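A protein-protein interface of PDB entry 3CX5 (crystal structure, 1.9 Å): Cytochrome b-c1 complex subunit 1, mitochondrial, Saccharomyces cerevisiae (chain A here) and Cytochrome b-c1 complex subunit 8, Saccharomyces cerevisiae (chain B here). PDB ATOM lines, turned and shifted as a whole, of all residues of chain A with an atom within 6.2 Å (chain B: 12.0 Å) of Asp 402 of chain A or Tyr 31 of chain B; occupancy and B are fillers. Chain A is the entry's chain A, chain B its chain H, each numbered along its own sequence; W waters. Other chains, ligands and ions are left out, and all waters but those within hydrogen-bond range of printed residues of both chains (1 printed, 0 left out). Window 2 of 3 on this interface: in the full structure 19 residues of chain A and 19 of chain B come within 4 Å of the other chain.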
ATOM      1  N   LEU A 400      -7.725 -17.365  21.695  1.00  0.00           N
ATOM      2  CA  LEU A 400      -8.396 -18.026  20.575  1.00  0.00           C
ATOM      3  C   LEU A 400      -9.005 -17.138  19.498  1.00  0.00           C
ATOM      4  O   LEU A 400      -8.745 -17.331  18.309  1.00  0.00           O
ATOM      5  CB  LEU A 400      -9.494 -18.945  21.125  1.00  0.00           C
ATOM      6  CG  LEU A 400      -9.336 -20.468  21.187  1.00  0.00           C
ATOM      7  CD1 LEU A 400      -7.910 -20.906  20.992  1.00  0.00           C
ATOM      8  CD2 LEU A 400      -9.895 -20.977  22.504  1.00  0.00           C
ATOM      9  N   TRP A 401      -9.837 -16.188  19.911  1.00  0.00           N
ATOM     10  CA  TRP A 401     -10.524 -15.314  18.974  1.00  0.00           C
ATOM     11  C   TRP A 401      -9.641 -14.521  18.025  1.00  0.00           C
ATOM     12  O   TRP A 401      -8.832 -13.694  18.451  1.00  0.00           O
ATOM     13  CB  TRP A 401     -11.473 -14.374  19.709  1.00  0.00           C
ATOM     14  CG  TRP A 401     -12.495 -13.742  18.799  1.00  0.00           C
ATOM     15  CD1 TRP A 401     -12.371 -12.572  18.108  1.00  0.00           C
ATOM     16  CD2 TRP A 401     -13.805 -14.240  18.513  1.00  0.00           C
ATOM     17  NE1 TRP A 401     -13.524 -12.306  17.414  1.00  0.00           N
ATOM     18  CE2 TRP A 401     -14.423 -13.313  17.646  1.00  0.00           C
ATOM     19  CE3 TRP A 401     -14.521 -15.380  18.909  1.00  0.00           C
ATOM     20  CZ2 TRP A 401     -15.725 -13.486  17.168  1.00  0.00           C
ATOM     21  CZ3 TRP A 401     -15.814 -15.551  18.433  1.00  0.00           C
ATOM     22  CH2 TRP A 401     -16.401 -14.605  17.571  1.00  0.00           C
ATOM     23  N   ASP A 402      -9.820 -14.785  16.730  1.00  0.00           N
ATOM     24  CA  ASP A 402      -9.072 -14.116  15.672  1.00  0.00           C
ATOM     25  C   ASP A 402      -7.558 -14.116  15.935  1.00  0.00           C
ATOM     26  O   ASP A 402      -6.876 -13.109  15.760  1.00  0.00           O
ATOM     27  CB  ASP A 402      -9.621 -12.694  15.472  1.00  0.00           C
ATOM     28  CG  ASP A 402      -9.098 -12.027  14.211  1.00  0.00           C
ATOM     29  OD1 ASP A 402      -8.640 -12.732  13.286  1.00  0.00           O
ATOM     30  OD2 ASP A 402      -9.142 -10.783  14.146  1.00  0.00           O
ATOM     31  N   GLN A 403      -7.042 -15.273  16.338  1.00  0.00           N
ATOM     32  CA  GLN A 403      -5.622 -15.433  16.617  1.00  0.00           C
ATOM     33  C   GLN A 403      -4.975 -16.395  15.635  1.00  0.00           C
ATOM     34  O   GLN A 403      -5.640 -17.284  15.099  1.00  0.00           O
ATOM     35  CB  GLN A 403      -5.405 -15.935  18.051  1.00  0.00           C
ATOM     36  CG  GLN A 403      -5.775 -14.919  19.123  1.00  0.00           C
ATOM     37  CD  GLN A 403      -5.037 -13.599  18.952  1.00  0.00           C
ATOM     38  OE1 GLN A 403      -3.810 -13.562  18.904  1.00  0.00           O
ATOM     39  NE2 GLN A 403      -5.791 -12.511  18.830  1.00  0.00           N
ATOM     40  N   ASP A 404      -3.678 -16.192  15.399  1.00  0.00           N
ATOM     41  CA  ASP A 404      -2.884 -17.030  14.507  1.00  0.00           C
ATOM     42  C   ASP A 404      -2.816 -18.469  15.008  1.00  0.00           C
ATOM     43  O   ASP A 404      -2.872 -18.733  16.219  1.00  0.00           O
ATOM     44  CB  ASP A 404      -1.457 -16.466  14.364  1.00  0.00           C
ATOM     45  CG  ASP A 404      -1.258 -15.655  13.077  1.00  0.00           C
ATOM     46  OD1 ASP A 404      -0.232 -14.957  12.956  1.00  0.00           O
ATOM     47  OD2 ASP A 404      -2.096 -15.739  12.161  1.00  0.00           O
ATOM     48  N   TYR A 419      -4.172 -22.402   4.534  1.00  0.00           N
ATOM     49  CA  TYR A 419      -4.030 -21.761   5.839  1.00  0.00           C
ATOM     50  C   TYR A 419      -5.120 -20.733   6.148  1.00  0.00           C
ATOM     51  O   TYR A 419      -5.755 -20.799   7.197  1.00  0.00           O
ATOM     52  CB  TYR A 419      -2.650 -21.096   5.963  1.00  0.00           C
ATOM     53  CG  TYR A 419      -2.372 -20.522   7.344  1.00  0.00           C
ATOM     54  CD1 TYR A 419      -1.830 -21.320   8.351  1.00  0.00           C
ATOM     55  CD2 TYR A 419      -2.690 -19.196   7.653  1.00  0.00           C
ATOM     56  CE1 TYR A 419      -1.610 -20.815   9.639  1.00  0.00           C
ATOM     57  CE2 TYR A 419      -2.473 -18.680   8.944  1.00  0.00           C
ATOM     58  CZ  TYR A 419      -1.933 -19.501   9.929  1.00  0.00           C
ATOM     59  OH  TYR A 419      -1.723 -19.013  11.212  1.00  0.00           O
ATOM     60  N   MET A 420      -5.337 -19.790   5.235  1.00  0.00           N
ATOM     61  CA  MET A 420      -6.330 -18.736   5.440  1.00  0.00           C
ATOM     62  C   MET A 420      -7.769 -19.183   5.669  1.00  0.00           C
ATOM     63  O   MET A 420      -8.485 -18.566   6.449  1.00  0.00           O
ATOM     64  CB  MET A 420      -6.228 -17.669   4.347  1.00  0.00           C
ATOM     65  CG  MET A 420      -5.011 -16.764   4.528  1.00  0.00           C
ATOM     66  SD  MET A 420      -5.010 -15.971   6.177  1.00  0.00           S
ATOM     67  CE  MET A 420      -5.671 -14.357   5.754  1.00  0.00           C
ATOM     68  N   ARG A 423      -7.603 -20.372   9.201  1.00  0.00           N
ATOM     69  CA  ARG A 423      -7.392 -19.203  10.059  1.00  0.00           C
ATOM     70  C   ARG A 423      -8.650 -18.328  10.185  1.00  0.00           C
ATOM     71  O   ARG A 423      -8.917 -17.765  11.251  1.00  0.00           O
ATOM     72  CB  ARG A 423      -6.194 -18.382   9.548  1.00  0.00           C
ATOM     73  CG  ARG A 423      -6.052 -16.969  10.136  1.00  0.00           C
ATOM     74  CD  ARG A 423      -5.703 -16.979  11.625  1.00  0.00           C
ATOM     75  NE  ARG A 423      -6.270 -15.811  12.315  1.00  0.00           N
ATOM     76  CZ  ARG A 423      -5.568 -14.739  12.663  1.00  0.00           C
ATOM     77  NH1 ARG A 423      -6.136 -13.720  13.277  1.00  0.00           N
ATOM     78  NH2 ARG A 423      -4.286 -14.684  12.392  1.00  0.00           N
ATOM     79  N   MET A 426     -11.261 -18.905  13.048  1.00  0.00           N
ATOM     80  CA  MET A 426     -10.935 -18.589  14.437  1.00  0.00           C
ATOM     81  C   MET A 426     -11.857 -17.509  14.986  1.00  0.00           C
ATOM     82  O   MET A 426     -11.689 -17.055  16.116  1.00  0.00           O
ATOM     83  CB  MET A 426      -9.469 -18.161  14.578  1.00  0.00           C
ATOM     84  CG  MET A 426      -8.477 -19.259  14.266  1.00  0.00           C
ATOM     85  SD  MET A 426      -8.751 -20.773  15.210  1.00  0.00           S
ATOM     86  CE  MET A 426      -8.171 -20.271  16.846  1.00  0.00           C
ATOM     87  N   SER A 427     -12.828 -17.096  14.176  1.00  0.00           N
ATOM     88  CA  SER A 427     -13.804 -16.085  14.575  1.00  0.00           C
ATOM     89  C   SER A 427     -15.111 -16.281  13.797  1.00  0.00           C
ATOM     90  O   SER A 427     -15.194 -17.132  12.916  1.00  0.00           O
ATOM     91  CB  SER A 427     -13.258 -14.673  14.331  1.00  0.00           C
ATOM     92  OG  SER A 427     -13.047 -14.424  12.951  1.00  0.00           O
ATOM     93  N   ALA B  27       4.509 -22.727   5.169  1.00  0.00           N
ATOM     94  CA  ALA B  27       3.920 -21.423   4.927  1.00  0.00           C
ATOM     95  C   ALA B  27       3.859 -20.676   6.241  1.00  0.00           C
ATOM     96  O   ALA B  27       3.904 -21.281   7.310  1.00  0.00           O
ATOM     97  CB  ALA B  27       2.498 -21.551   4.318  1.00  0.00           C
ATOM     98  N   VAL B  28       3.752 -19.359   6.138  1.00  0.00           N
ATOM     99  CA  VAL B  28       3.681 -18.485   7.297  1.00  0.00           C
ATOM    100  C   VAL B  28       2.433 -17.623   7.174  1.00  0.00           C
ATOM    101  O   VAL B  28       2.051 -17.221   6.077  1.00  0.00           O
ATOM    102  CB  VAL B  28       4.941 -17.574   7.378  1.00  0.00           C
ATOM    103  CG1 VAL B  28       4.766 -16.510   8.447  1.00  0.00           C
ATOM    104  CG2 VAL B  28       6.166 -18.410   7.685  1.00  0.00           C
ATOM    105  N   SER B  29       1.796 -17.342   8.301  1.00  0.00           N
ATOM    106  CA  SER B  29       0.593 -16.527   8.295  1.00  0.00           C
ATOM    107  C   SER B  29       0.795 -15.116   7.740  1.00  0.00           C
ATOM    108  O   SER B  29       1.813 -14.471   8.012  1.00  0.00           O
ATOM    109  CB  SER B  29       0.036 -16.411   9.710  1.00  0.00           C
ATOM    110  OG  SER B  29      -1.058 -15.507   9.730  1.00  0.00           O
ATOM    111  N   PRO B  30      -0.166 -14.634   6.929  1.00  0.00           N
ATOM    112  CA  PRO B  30      -0.111 -13.294   6.339  1.00  0.00           C
ATOM    113  C   PRO B  30      -0.059 -12.243   7.455  1.00  0.00           C
ATOM    114  O   PRO B  30       0.482 -11.161   7.267  1.00  0.00           O
ATOM    115  CB  PRO B  30      -1.434 -13.209   5.578  1.00  0.00           C
ATOM    116  CG  PRO B  30      -1.647 -14.602   5.130  1.00  0.00           C
ATOM    117  CD  PRO B  30      -1.294 -15.401   6.370  1.00  0.00           C
ATOM    118  N   TYR B  31      -0.628 -12.576   8.613  1.00  0.00           N
ATOM    119  CA  TYR B  31      -0.640 -11.669   9.765  1.00  0.00           C
ATOM    120  C   TYR B  31       0.756 -11.459  10.348  1.00  0.00           C
ATOM    121  O   TYR B  31       1.019 -10.434  10.976  1.00  0.00           O
ATOM    122  CB  TYR B  31      -1.533 -12.215  10.874  1.00  0.00           C
ATOM    123  CG  TYR B  31      -3.015 -12.144  10.598  1.00  0.00           C
ATOM    124  CD1 TYR B  31      -3.655 -13.132   9.847  1.00  0.00           C
ATOM    125  CD2 TYR B  31      -3.789 -11.117  11.134  1.00  0.00           C
ATOM    126  CE1 TYR B  31      -5.036 -13.103   9.646  1.00  0.00           C
ATOM    127  CE2 TYR B  31      -5.166 -11.076  10.937  1.00  0.00           C
ATOM    128  CZ  TYR B  31      -5.782 -12.079  10.195  1.00  0.00           C
ATOM    129  OH  TYR B  31      -7.142 -12.066  10.037  1.00  0.00           O
ATOM    130  N   ALA B  32       1.624 -12.455  10.173  1.00  0.00           N
ATOM    131  CA  ALA B  32       2.993 -12.406  10.682  1.00  0.00           C
ATOM    132  C   ALA B  32       3.993 -11.825   9.684  1.00  0.00           C
ATOM    133  O   ALA B  32       5.178 -11.705   9.988  1.00  0.00           O
ATOM    134  CB  ALA B  32       3.439 -13.802  11.102  1.00  0.00           C
ATOM    135  N   GLN B  33       3.519 -11.466   8.495  1.00  0.00           N
ATOM    136  CA  GLN B  33       4.397 -10.919   7.466  1.00  0.00           C
ATOM    137  C   GLN B  33       4.385  -9.396   7.422  1.00  0.00           C
ATOM    138  O   GLN B  33       3.498  -8.754   7.986  1.00  0.00           O
ATOM    139  CB  GLN B  33       4.025 -11.492   6.097  1.00  0.00           C
ATOM    140  CG  GLN B  33       4.100 -13.010   6.030  1.00  0.00           C
ATOM    141  CD  GLN B  33       3.776 -13.562   4.651  1.00  0.00           C
ATOM    142  OE1 GLN B  33       4.089 -12.942   3.634  1.00  0.00           O
ATOM    143  NE2 GLN B  33       3.146 -14.733   4.611  1.00  0.00           N
ATOM    144  N   LYS B  34       5.407  -8.827   6.787  1.00  0.00           N
ATOM    145  CA  LYS B  34       5.532  -7.381   6.641  1.00  0.00           C
ATOM    146  C   LYS B  34       4.349  -6.895   5.819  1.00  0.00           C
ATOM    147  O   LYS B  34       4.111  -7.398   4.723  1.00  0.00           O
ATOM    148  CB  LYS B  34       6.842  -7.037   5.931  1.00  0.00           C
ATOM    149  CG  LYS B  34       8.069  -7.209   6.803  1.00  0.00           C
ATOM    150  CD  LYS B  34       9.277  -7.650   5.996  1.00  0.00           C
ATOM    151  CE  LYS B  34       9.616  -6.673   4.888  1.00  0.00           C
ATOM    152  NZ  LYS B  34      10.809  -7.146   4.132  1.00  0.00           N
ATOM    153  N   PRO B  35       3.589  -5.920   6.349  1.00  0.00           N
ATOM    154  CA  PRO B  35       2.400  -5.310   5.738  1.00  0.00           C
ATOM    155  C   PRO B  35       2.565  -4.738   4.329  1.00  0.00           C
ATOM    156  O   PRO B  35       2.180  -3.597   4.056  1.00  0.00           O
ATOM    157  CB  PRO B  35       2.006  -4.233   6.755  1.00  0.00           C
ATOM    158  CG  PRO B  35       3.296  -3.901   7.433  1.00  0.00           C
ATOM    159  CD  PRO B  35       3.902  -5.260   7.629  1.00  0.00           C
ATOM    160  N   LEU B  36       3.103  -5.562   3.432  1.00  0.00           N
ATOM    161  CA  LEU B  36       3.323  -5.195   2.036  1.00  0.00           C
ATOM    162  C   LEU B  36       4.058  -3.863   1.908  1.00  0.00           C
ATOM    163  O   LEU B  36       3.730  -3.029   1.064  1.00  0.00           O
ATOM    164  CB  LEU B  36       1.983  -5.167   1.296  1.00  0.00           C
ATOM    165  CG  LEU B  36       1.171  -6.459   1.463  1.00  0.00           C
ATOM    166  CD1 LEU B  36      -0.257  -6.250   0.992  1.00  0.00           C
ATOM    167  CD2 LEU B  36       1.841  -7.610   0.723  1.00  0.00           C
ATOM    168  N   GLN B  37       5.044  -3.673   2.782  1.00  0.00           N
ATOM    169  CA  GLN B  37       5.857  -2.463   2.804  1.00  0.00           C
ATOM    170  C   GLN B  37       7.115  -2.643   1.952  1.00  0.00           C
ATOM    171  O   GLN B  37       8.237  -2.395   2.402  1.00  0.00           O
ATOM    172  CB  GLN B  37       6.210  -2.095   4.252  1.00  0.00           C
ATOM    173  CG  GLN B  37       6.674  -3.272   5.108  1.00  0.00           C
ATOM    174  CD  GLN B  37       6.671  -2.956   6.595  1.00  0.00           C
ATOM    175  OE1 GLN B  37       5.935  -2.081   7.058  1.00  0.00           O
ATOM    176  NE2 GLN B  37       7.486  -3.680   7.353  1.00  0.00           N
HETATM  177  O   HOH W   1      -9.184 -14.007  10.217  1.00  0.00           O
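Asp 402 of chain A touches just one residue of chain B: Tyr 31. Tyr 31 of chain B touches just these residues of chain A: Asp 402, Asp 404 and Arg 423. No residue of chain B comes within 4 Å of Trp 401 of chain A. Of the printed residues of chain B, Asp 404 of chain A touches Ser 29 (2.7 Å) and Tyr 31 (3.7 Å). Arg 423 of chain A touches just one residue of chain B: Tyr 31 (3.0 Å). No residue of chain B comes within 4 Å of Met 426 of chain A. No residue of chain B comes within 4 Å of Ser 427 of chain A. Printed residues of chain A within 4 Å of Pro 30 of chain B: Met 420. Printed residues of chain B within 4 Å of Met 420 of chain A: Pro 30 (3.8 Å). The nearest residue of chain B that does not touch Asp 402 of chain A is Ser 29 of chain B (8.7 Å). The nearest printed residue of chain B that does not touch Tyr 419 of chain A is Pro 30 of chain B (4.2 Å).
The side-chain carboxylate of Asp 404 of chain A is in hydrogen-bond range of the side-chain hydroxyl of Tyr 419 of chain A. The guanidinium group of Arg 423 of chain A is in salt-bridge range of the side-chain carboxylate of Asp 402 of chain A (2.7 Å). The guanidinium group (NH2) of Arg 423 of chain A is in salt-bridge range of the side-chain carboxylate (OD2) of Asp 404 of chain A (2.4 Å). The backbone carbonyl oxygen (O) of Met 426 of chain A lies within hydrogen-bond range of the backbone NH (N) of Asp 402 of chain A. The guanidinium group of Arg 423 of chain A lies within hydrogen-bond range of the backbone carbonyl oxygen of Gln 403 of chain A (3.2 Å). The side-chain hydroxyl (OG) of Ser 29 of chain B sits close to the backbone NH (N) of Tyr 31 of chain B, 3.2 Å away.
Hydrophobic or aromatic side chains of chain A within 4 Å of the printed part of chain B: Tyr 419 and Met 420. Among the printed residues, 6 pairs touch across the chains.
Among the printed residues, merely in contact across the chains: Arg 423 of chain A with Tyr 31 of chain B (3.0 Å), Tyr 419 of chain A with Ser 29 of chain B (3.5 Å), Asp 402 of chain A with Tyr 31 of chain B (3.6 Å), Asp 404 of chain A with Tyr 31 of chain B (3.7 Å) and Met 420 of chain A with Pro 30 of chain B (3.8 Å).
OG of Ser 29 of chain B lies within hydrogen-bond range of OD2 of Asp 404 of chain A (2.7 Å).
Water W1 bridges OH of Tyr 31 of chain B (2.8 Å) and OD1 of Asp 402 of chain A (3.4 Å).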
